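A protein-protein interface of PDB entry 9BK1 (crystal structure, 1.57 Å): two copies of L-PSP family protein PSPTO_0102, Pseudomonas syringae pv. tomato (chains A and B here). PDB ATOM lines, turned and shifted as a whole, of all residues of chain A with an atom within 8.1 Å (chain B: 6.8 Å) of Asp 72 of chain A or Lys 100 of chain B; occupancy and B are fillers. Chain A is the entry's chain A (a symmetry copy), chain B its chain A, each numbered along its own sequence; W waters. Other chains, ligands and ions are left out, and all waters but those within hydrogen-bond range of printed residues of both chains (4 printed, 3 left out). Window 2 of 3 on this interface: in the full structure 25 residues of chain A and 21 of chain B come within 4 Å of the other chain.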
ATOM      1  N   ILE A  66       1.679  -4.539 -11.204  1.00  0.00           N
ATOM      2  CA  ILE A  66       2.092  -3.376 -10.433  1.00  0.00           C
ATOM      3  C   ILE A  66       1.111  -2.259 -10.728  1.00  0.00           C
ATOM      4  O   ILE A  66       0.924  -1.897 -11.895  1.00  0.00           O
ATOM      5  CB  ILE A  66       3.513  -2.934 -10.806  1.00  0.00           C
ATOM      6  CG1 ILE A  66       4.506  -4.058 -10.506  1.00  0.00           C
ATOM      7  CG2 ILE A  66       3.894  -1.663 -10.056  1.00  0.00           C
ATOM      8  CD1 ILE A  66       5.895  -3.819 -11.038  1.00  0.00           C
ATOM      9  N   LEU A  68       0.277   1.741  -9.991  1.00  0.00           N
ATOM     10  CA  LEU A  68       0.853   3.012  -9.571  1.00  0.00           C
ATOM     11  C   LEU A  68      -0.241   4.061  -9.508  1.00  0.00           C
ATOM     12  O   LEU A  68      -1.089   4.140 -10.404  1.00  0.00           O
ATOM     13  CB  LEU A  68       1.962   3.484 -10.522  1.00  0.00           C
ATOM     14  CG  LEU A  68       3.251   2.665 -10.501  1.00  0.00           C
ATOM     15  CD1 LEU A  68       4.157   2.979 -11.696  1.00  0.00           C
ATOM     16  CD2 LEU A  68       3.998   2.914  -9.183  1.00  0.00           C
ATOM     17  N   LYS A  69      -0.206   4.881  -8.457  1.00  0.00           N
ATOM     18  CA  LYS A  69      -1.155   5.989  -8.359  1.00  0.00           C
ATOM     19  C   LYS A  69      -0.993   6.958  -9.524  1.00  0.00           C
ATOM     20  O   LYS A  69      -1.986   7.440 -10.083  1.00  0.00           O
ATOM     21  CB  LYS A  69      -0.977   6.727  -7.034  1.00  0.00           C
ATOM     22  CG  LYS A  69      -1.873   7.958  -6.894  1.00  0.00           C
ATOM     23  CD  LYS A  69      -1.583   8.719  -5.610  1.00  0.00           C
ATOM     24  CE  LYS A  69      -2.204  10.101  -5.642  1.00  0.00           C
ATOM     25  NZ  LYS A  69      -1.783  10.866  -4.430  1.00  0.00           N
ATOM     26  N   ASP A  70       0.248   7.245  -9.909  1.00  0.00           N
ATOM     27  CA  ASP A  70       0.559   8.194 -10.982  1.00  0.00           C
ATOM     28  C   ASP A  70       1.669   7.561 -11.813  1.00  0.00           C
ATOM     29  O   ASP A  70       2.839   7.651 -11.440  1.00  0.00           O
ATOM     30  CB  ASP A  70       0.984   9.537 -10.393  1.00  0.00           C
ATOM     31  CG  ASP A  70       1.171  10.621 -11.445  1.00  0.00           C
ATOM     32  OD1 ASP A  70       1.542  10.308 -12.594  1.00  0.00           O
ATOM     33  OD2 ASP A  70       0.958  11.805 -11.102  1.00  0.00           O
ATOM     34  N   ILE A  71       1.312   6.910 -12.922  1.00  0.00           N
ATOM     35  CA  ILE A  71       2.327   6.168 -13.667  1.00  0.00           C
ATOM     36  C   ILE A  71       3.323   7.120 -14.326  1.00  0.00           C
ATOM     37  O   ILE A  71       4.532   6.845 -14.355  1.00  0.00           O
ATOM     38  CB  ILE A  71       1.664   5.199 -14.670  1.00  0.00           C
ATOM     39  CG1 ILE A  71       2.701   4.228 -15.256  1.00  0.00           C
ATOM     40  CG2 ILE A  71       0.936   5.948 -15.787  1.00  0.00           C
ATOM     41  CD1 ILE A  71       2.087   2.894 -15.705  1.00  0.00           C
ATOM     42  N   ASP A  72       2.854   8.283 -14.793  1.00  0.00           N
ATOM     43  CA  ASP A  72       3.774   9.253 -15.382  1.00  0.00           C
ATOM     44  C   ASP A  72       4.800   9.733 -14.363  1.00  0.00           C
ATOM     45  O   ASP A  72       5.990   9.847 -14.678  1.00  0.00           O
ATOM     46  CB  ASP A  72       3.003  10.443 -15.960  1.00  0.00           C
ATOM     47  CG  ASP A  72       2.219  10.083 -17.197  1.00  0.00           C
ATOM     48  OD1 ASP A  72       2.649   9.167 -17.930  1.00  0.00           O
ATOM     49  OD2 ASP A  72       1.170  10.718 -17.438  1.00  0.00           O
ATOM     50  N   ALA A  73       4.361  10.018 -13.133  1.00  0.00           N
ATOM     51  CA  ALA A  73       5.292  10.529 -12.133  1.00  0.00           C
ATOM     52  C   ALA A  73       6.254   9.450 -11.648  1.00  0.00           C
ATOM     53  O   ALA A  73       7.444   9.718 -11.448  1.00  0.00           O
ATOM     54  CB  ALA A  73       4.531  11.115 -10.942  1.00  0.00           C
ATOM     55  N   ASP A  74       5.765   8.227 -11.443  1.00  0.00           N
ATOM     56  CA  ASP A  74       6.467   7.281 -10.587  1.00  0.00           C
ATOM     57  C   ASP A  74       6.928   5.998 -11.265  1.00  0.00           C
ATOM     58  O   ASP A  74       7.553   5.166 -10.589  1.00  0.00           O
ATOM     59  CB  ASP A  74       5.588   6.919  -9.387  1.00  0.00           C
ATOM     60  CG  ASP A  74       5.440   8.063  -8.409  1.00  0.00           C
ATOM     61  OD1 ASP A  74       6.419   8.829  -8.251  1.00  0.00           O
ATOM     62  OD2 ASP A  74       4.361   8.197  -7.793  1.00  0.00           O
ATOM     63  N   PHE A  75       6.647   5.809 -12.558  1.00  0.00           N
ATOM     64  CA  PHE A  75       7.110   4.614 -13.261  1.00  0.00           C
ATOM     65  C   PHE A  75       8.619   4.450 -13.129  1.00  0.00           C
ATOM     66  O   PHE A  75       9.113   3.373 -12.780  1.00  0.00           O
ATOM     67  CB  PHE A  75       6.690   4.707 -14.728  1.00  0.00           C
ATOM     68  CG  PHE A  75       7.024   3.492 -15.567  1.00  0.00           C
ATOM     69  CD1 PHE A  75       6.509   2.239 -15.253  1.00  0.00           C
ATOM     70  CD2 PHE A  75       7.797   3.621 -16.710  1.00  0.00           C
ATOM     71  CE1 PHE A  75       6.787   1.136 -16.047  1.00  0.00           C
ATOM     72  CE2 PHE A  75       8.078   2.523 -17.510  1.00  0.00           C
ATOM     73  CZ  PHE A  75       7.567   1.277 -17.172  1.00  0.00           C
ATOM     74  N   ALA A  76       9.370   5.529 -13.365  1.00  0.00           N
ATOM     75  CA  ALA A  76      10.823   5.402 -13.385  1.00  0.00           C
ATOM     76  C   ALA A  76      11.374   5.133 -11.990  1.00  0.00           C
ATOM     77  O   ALA A  76      12.291   4.317 -11.820  1.00  0.00           O
ATOM     78  CB  ALA A  76      11.446   6.664 -13.986  1.00  0.00           C
ATOM     79  N   GLY A  77      10.830   5.807 -10.978  1.00  0.00           N
ATOM     80  CA  GLY A  77      11.294   5.573  -9.620  1.00  0.00           C
ATOM     81  C   GLY A  77      10.989   4.170  -9.138  1.00  0.00           C
ATOM     82  O   GLY A  77      11.827   3.525  -8.498  1.00  0.00           O
ATOM     83  N   THR A  96       2.433  -3.253 -15.583  1.00  0.00           N
ATOM     84  CA  THR A  96       2.435  -2.040 -14.767  1.00  0.00           C
ATOM     85  C   THR A  96       1.414  -1.061 -15.337  1.00  0.00           C
ATOM     86  O   THR A  96       1.494  -0.694 -16.515  1.00  0.00           O
ATOM     87  CB  THR A  96       3.831  -1.409 -14.754  1.00  0.00           C
ATOM     88  OG1 THR A  96       4.787  -2.379 -14.306  1.00  0.00           O
ATOM     89  CG2 THR A  96       3.880  -0.204 -13.842  1.00  0.00           C
ATOM     90  N   VAL A  97       0.453  -0.639 -14.505  1.00  0.00           N
ATOM     91  CA  VAL A  97      -0.635   0.226 -14.960  1.00  0.00           C
ATOM     92  C   VAL A  97      -0.941   1.263 -13.888  1.00  0.00           C
ATOM     93  O   VAL A  97      -0.552   1.125 -12.728  1.00  0.00           O
ATOM     94  CB  VAL A  97      -1.925  -0.561 -15.307  1.00  0.00           C
ATOM     95  CG1 VAL A  97      -1.617  -1.692 -16.279  1.00  0.00           C
ATOM     96  CG2 VAL A  97      -2.566  -1.127 -14.039  1.00  0.00           C
ATOM     97  N   GLU A  98      -1.665   2.308 -14.285  1.00  0.00           N
ATOM     98  CA  GLU A  98      -2.062   3.341 -13.338  1.00  0.00           C
ATOM     99  C   GLU A  98      -3.433   3.014 -12.758  1.00  0.00           C
ATOM    100  O   GLU A  98      -4.425   2.916 -13.494  1.00  0.00           O
ATOM    101  CB  GLU A  98      -2.082   4.727 -13.977  1.00  0.00           C
ATOM    102  CG  GLU A  98      -2.423   5.793 -12.944  1.00  0.00           C
ATOM    103  CD  GLU A  98      -2.362   7.186 -13.502  1.00  0.00           C
ATOM    104  OE1 GLU A  98      -1.278   7.568 -13.988  1.00  0.00           O
ATOM    105  OE2 GLU A  98      -3.392   7.898 -13.450  1.00  0.00           O
ATOM    106  N   ALA A  99      -3.483   2.859 -11.438  1.00  0.00           N
ATOM    107  CA  ALA A  99      -4.739   2.662 -10.731  1.00  0.00           C
ATOM    108  C   ALA A  99      -4.574   3.197  -9.319  1.00  0.00           C
ATOM    109  O   ALA A  99      -3.673   2.759  -8.592  1.00  0.00           O
ATOM    110  CB  ALA A  99      -5.124   1.179 -10.720  1.00  0.00           C
ATOM    111  N   TYR B  67      -6.319  -3.653 -20.318  1.00  0.00           N
ATOM    112  CA  TYR B  67      -6.237  -2.294 -19.798  1.00  0.00           C
ATOM    113  C   TYR B  67      -6.340  -1.316 -20.955  1.00  0.00           C
ATOM    114  O   TYR B  67      -5.591  -1.427 -21.929  1.00  0.00           O
ATOM    115  CB  TYR B  67      -4.921  -2.075 -19.052  1.00  0.00           C
ATOM    116  CG  TYR B  67      -4.650  -3.084 -17.958  1.00  0.00           C
ATOM    117  CD1 TYR B  67      -5.239  -2.954 -16.702  1.00  0.00           C
ATOM    118  CD2 TYR B  67      -3.798  -4.164 -18.180  1.00  0.00           C
ATOM    119  CE1 TYR B  67      -4.995  -3.865 -15.707  1.00  0.00           C
ATOM    120  CE2 TYR B  67      -3.550  -5.087 -17.191  1.00  0.00           C
ATOM    121  CZ  TYR B  67      -4.143  -4.935 -15.953  1.00  0.00           C
ATOM    122  OH  TYR B  67      -3.886  -5.851 -14.960  1.00  0.00           O
ATOM    123  N   LEU B  68      -7.241  -0.343 -20.832  1.00  0.00           N
ATOM    124  CA  LEU B  68      -7.412   0.699 -21.837  1.00  0.00           C
ATOM    125  C   LEU B  68      -7.095   2.047 -21.218  1.00  0.00           C
ATOM    126  O   LEU B  68      -7.507   2.334 -20.087  1.00  0.00           O
ATOM    127  CB  LEU B  68      -8.837   0.720 -22.407  1.00  0.00           C
ATOM    128  CG  LEU B  68      -9.221  -0.468 -23.287  1.00  0.00           C
ATOM    129  CD1 LEU B  68     -10.731  -0.548 -23.528  1.00  0.00           C
ATOM    130  CD2 LEU B  68      -8.468  -0.383 -24.622  1.00  0.00           C
ATOM    131  N   LYS B  69      -6.378   2.883 -21.971  1.00  0.00           N
ATOM    132  CA  LYS B  69      -6.109   4.243 -21.505  1.00  0.00           C
ATOM    133  C   LYS B  69      -7.402   5.024 -21.305  1.00  0.00           C
ATOM    134  O   LYS B  69      -7.545   5.761 -20.322  1.00  0.00           O
ATOM    135  CB  LYS B  69      -5.201   4.973 -22.492  1.00  0.00           C
ATOM    136  CG  LYS B  69      -4.945   6.434 -22.121  1.00  0.00           C
ATOM    137  CD  LYS B  69      -4.129   7.148 -23.188  1.00  0.00           C
ATOM    138  CE  LYS B  69      -4.179   8.650 -22.999  1.00  0.00           C
ATOM    139  NZ  LYS B  69      -3.484   9.321 -24.139  1.00  0.00           N
ATOM    140  N   ASP B  70      -8.356   4.866 -22.219  1.00  0.00           N
ATOM    141  CA  ASP B  70      -9.631   5.587 -22.184  1.00  0.00           C
ATOM    142  C   ASP B  70     -10.713   4.573 -22.541  1.00  0.00           C
ATOM    143  O   ASP B  70     -10.935   4.305 -23.721  1.00  0.00           O
ATOM    144  CB  ASP B  70      -9.605   6.758 -23.164  1.00  0.00           C
ATOM    145  CG  ASP B  70     -10.836   7.646 -23.070  1.00  0.00           C
ATOM    146  OD1 ASP B  70     -11.930   7.152 -22.733  1.00  0.00           O
ATOM    147  OD2 ASP B  70     -10.701   8.857 -23.357  1.00  0.00           O
ATOM    148  N   GLU B  98     -10.212   0.522 -17.233  1.00  0.00           N
ATOM    149  CA  GLU B  98      -9.439   1.691 -17.628  1.00  0.00           C
ATOM    150  C   GLU B  98      -8.249   1.867 -16.692  1.00  0.00           C
ATOM    151  O   GLU B  98      -8.419   2.044 -15.477  1.00  0.00           O
ATOM    152  CB  GLU B  98     -10.285   2.962 -17.641  1.00  0.00           C
ATOM    153  CG  GLU B  98      -9.469   4.150 -18.133  1.00  0.00           C
ATOM    154  CD  GLU B  98     -10.283   5.405 -18.255  1.00  0.00           C
ATOM    155  OE1 GLU B  98     -11.275   5.382 -19.012  1.00  0.00           O
ATOM    156  OE2 GLU B  98      -9.931   6.414 -17.600  1.00  0.00           O
ATOM    157  N   ALA B  99      -7.049   1.828 -17.264  1.00  0.00           N
ATOM    158  CA  ALA B  99      -5.829   2.098 -16.518  1.00  0.00           C
ATOM    159  C   ALA B  99      -4.796   2.647 -17.488  1.00  0.00           C
ATOM    160  O   ALA B  99      -4.476   1.993 -18.488  1.00  0.00           O
ATOM    161  CB  ALA B  99      -5.324   0.823 -15.833  1.00  0.00           C
ATOM    162  N   LYS B 100      -4.270   3.835 -17.188  1.00  0.00           N
ATOM    163  CA  LYS B 100      -3.236   4.430 -18.030  1.00  0.00           C
ATOM    164  C   LYS B 100      -2.011   3.523 -18.091  1.00  0.00           C
ATOM    165  O   LYS B 100      -1.604   2.921 -17.086  1.00  0.00           O
ATOM    166  CB  LYS B 100      -2.825   5.804 -17.492  1.00  0.00           C
ATOM    167  CG  LYS B 100      -3.831   6.923 -17.713  1.00  0.00           C
ATOM    168  CD  LYS B 100      -3.342   8.229 -17.087  1.00  0.00           C
ATOM    169  CE  LYS B 100      -1.876   8.471 -17.411  1.00  0.00           C
ATOM    170  NZ  LYS B 100      -1.428   9.845 -17.041  1.00  0.00           N
ATOM    171  N   LEU B 101      -1.434   3.413 -19.283  1.00  0.00           N
ATOM    172  CA  LEU B 101      -0.214   2.647 -19.466  1.00  0.00           C
ATOM    173  C   LEU B 101       0.986   3.591 -19.351  1.00  0.00           C
ATOM    174  O   LEU B 101       0.842   4.794 -19.110  1.00  0.00           O
ATOM    175  CB  LEU B 101      -0.264   1.888 -20.796  1.00  0.00           C
ATOM    176  CG  LEU B 101      -1.406   0.858 -20.945  1.00  0.00           C
ATOM    177  CD1 LEU B 101      -1.631   0.077 -19.641  1.00  0.00           C
ATOM    178  CD2 LEU B 101      -2.721   1.469 -21.415  1.00  0.00           C
ATOM    179  N   CYS B 102       2.193   3.043 -19.503  1.00  0.00           N
ATOM    180  CA  CYS B 102       3.362   3.795 -19.058  1.00  0.00           C
ATOM    181  C   CYS B 102       3.729   4.941 -19.992  1.00  0.00           C
ATOM    182  O   CYS B 102       4.548   5.783 -19.610  1.00  0.00           O
ATOM    183  CB  CYS B 102       4.556   2.861 -18.875  1.00  0.00           C
ATOM    184  SG  CYS B 102       5.198   2.167 -20.386  1.00  0.00           S
ATOM    185  N   GLU B 103       3.139   5.008 -21.183  1.00  0.00           N
ATOM    186  CA  GLU B 103       3.309   6.147 -22.073  1.00  0.00           C
ATOM    187  C   GLU B 103       1.946   6.591 -22.589  1.00  0.00           C
ATOM    188  O   GLU B 103       1.075   5.751 -22.838  1.00  0.00           O
ATOM    189  CB  GLU B 103       4.225   5.796 -23.254  1.00  0.00           C
ATOM    190  CG  GLU B 103       5.577   5.256 -22.846  1.00  0.00           C
ATOM    191  CD  GLU B 103       6.679   6.266 -23.032  1.00  0.00           C
ATOM    192  OE1 GLU B 103       6.460   7.247 -23.779  1.00  0.00           O
ATOM    193  OE2 GLU B 103       7.764   6.081 -22.435  1.00  0.00           O
ATOM    194  N   PRO B 104       1.729   7.895 -22.765  1.00  0.00           N
ATOM    195  CA  PRO B 104       0.387   8.363 -23.149  1.00  0.00           C
ATOM    196  C   PRO B 104      -0.095   7.848 -24.501  1.00  0.00           C
ATOM    197  O   PRO B 104      -1.313   7.763 -24.716  1.00  0.00           O
ATOM    198  CB  PRO B 104       0.534   9.897 -23.144  1.00  0.00           C
ATOM    199  CG  PRO B 104       1.994  10.151 -23.227  1.00  0.00           C
ATOM    200  CD  PRO B 104       2.653   9.011 -22.506  1.00  0.00           C
ATOM    201  N   ILE B 106       0.218   4.815 -25.597  1.00  0.00           N
ATOM    202  CA  ILE B 106      -0.200   3.422 -25.499  1.00  0.00           C
ATOM    203  C   ILE B 106      -1.675   3.394 -25.116  1.00  0.00           C
ATOM    204  O   ILE B 106      -2.057   3.888 -24.052  1.00  0.00           O
ATOM    205  CB  ILE B 106       0.661   2.659 -24.482  1.00  0.00           C
ATOM    206  CG1 ILE B 106       2.130   2.656 -24.923  1.00  0.00           C
ATOM    207  CG2 ILE B 106       0.122   1.235 -24.290  1.00  0.00           C
ATOM    208  CD1 ILE B 106       3.075   2.020 -23.924  1.00  0.00           C
ATOM    209  N   GLU B 109      -3.262  -2.500 -23.353  1.00  0.00           N
ATOM    210  CA  GLU B 109      -2.275  -3.464 -22.880  1.00  0.00           C
ATOM    211  C   GLU B 109      -3.002  -4.713 -22.419  1.00  0.00           C
ATOM    212  O   GLU B 109      -4.044  -4.616 -21.765  1.00  0.00           O
ATOM    213  CB  GLU B 109      -1.428  -2.898 -21.731  1.00  0.00           C
ATOM    214  CG  GLU B 109      -0.386  -3.887 -21.189  1.00  0.00           C
ATOM    215  CD  GLU B 109       0.701  -3.246 -20.346  1.00  0.00           C
ATOM    216  OE1 GLU B 109       0.933  -2.017 -20.449  1.00  0.00           O
ATOM    217  OE2 GLU B 109       1.347  -3.978 -19.564  1.00  0.00           O
HETATM  218  O   HOH W   1       5.724   6.854 -17.266  1.00  0.00           O
HETATM  219  O   HOH W   2       3.487  -3.168 -18.482  1.00  0.00           O
HETATM  220  O   HOH W   3       2.132   0.063 -19.030  1.00  0.00           O
HETATM  221  O   HOH W   4       1.073   7.468 -19.577  1.00  0.00           O
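Of the 15 printed residues of chain A, 5 touch a printed residue of chain B.
Along chain B the printed residues that touch a printed residue of chain A span positions 67 to 102.
Among the printed residues, pairs that only touch across the chains: Ile 71 of chain A with Lys 100 of chain B, Ile 71 of chain A with Leu 101 of chain B, Ile 71 of chain A with Cys 102 of chain B, Phe 75 of chain A with Cys 102 of chain B, Val 97 of chain A with Tyr 67 of chain B, Val 97 of chain A with Ala 99 of chain B, Val 97 of chain A with Lys 100 of chain B, Val 97 of chain A with Leu 101 of chain B and Glu 98 of chain A with Ala 99 of chain B.
The side-chain carboxylate of Asp 72 of chain A is in salt-bridge range of the side-chain amino group of Lys 100 of chain B, at 2.8 Å.
The side-chain amino group (NZ) of Lys 100 of chain B lies within salt-bridge range of the side-chain carboxylate (OE1) of Glu 98 of chain A.
The backbone NH of Ile 71 of chain A sits at hydrogen-bond distance from the side-chain carboxylate of Glu 98 of chain A (2.9 Å).
O of Leu 68 of chain B lies within hydrogen-bond range of N of Ala 99 of chain B (2.9 Å).
The side-chain carboxylate (OD1) of Asp 70 of chain A sits at hydrogen-bond distance from the backbone NH (N) of Asp 72 of chain A (3.3 Å).
N of Tyr 67 of chain B lies within hydrogen-bond range of O of Glu 109 of chain B, 2.9 Å away.
N of Val 97 of chain A lies within hydrogen-bond range of O of Ile 66 of chain A (2.9 Å).
The backbone NH of Leu 68 of chain A sits at hydrogen-bond distance from the backbone carbonyl oxygen of Val 97 of chain A (2.9 Å).
Glu 98 of chain A touches Ala 99 of chain B, but with the chains exchanged Ala 99 of chain A does not touch Glu 98 of chain B (5.9 Å).
Water W2 lies within hydrogen-bond range of the side-chain carboxylate (OE2) of Glu 109 of chain B (2.5 Å) and the backbone NH (N) of Thr 96 of chain A (3.1 Å).
Water W3 lies within hydrogen-bond range of the backbone carbonyl oxygen of Thr 96 of chain A, the side-chain carboxylate of Glu 109 of chain B and the backbone NH of Cys 102 of chain B.
Water W4 lies within hydrogen-bond range of the backbone carbonyl oxygen of Leu 101 of chain B and the side-chain carboxylate of Asp 72 of chain A.
Water W1 lies within hydrogen-bond range of O of Cys 102 of chain B (2.8 Å) and O of Ile 71 of chain A (3.1 Å).
Asp 72 of chain A touches one residue of chain B.
Of chain A, only Ile 71, Asp 72, Val 97 and Glu 98 come within 4 Å of Lys 100 of chain B.
Of the printed residues of chain A, Ala 99 of chain B touches Val 97 and Glu 98.
Printed residues of chain A within 4 Å of Leu 101 of chain B: Ile 71 (3.5 Å) and Val 97 (3.8 Å).
Printed residues of chain B within 4 Å of Glu 98 of chain A: Ala 99 (3.3 Å) and Lys 100 (2.9 Å).
Of the printed residues of chain B, Val 97 of chain A touches Tyr 67 (3.7 Å), Ala 99 (3.7 Å), Lys 100 (3.6 Å) and Leu 101 (3.8 Å).
The nearest residue of chain A that does not touch Lys 100 of chain B is Thr 96 of chain A (4.8 Å).
The nearest printed residue of chain B that does not touch Phe 75 of chain A is Glu 103 of chain B (6.1 Å).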
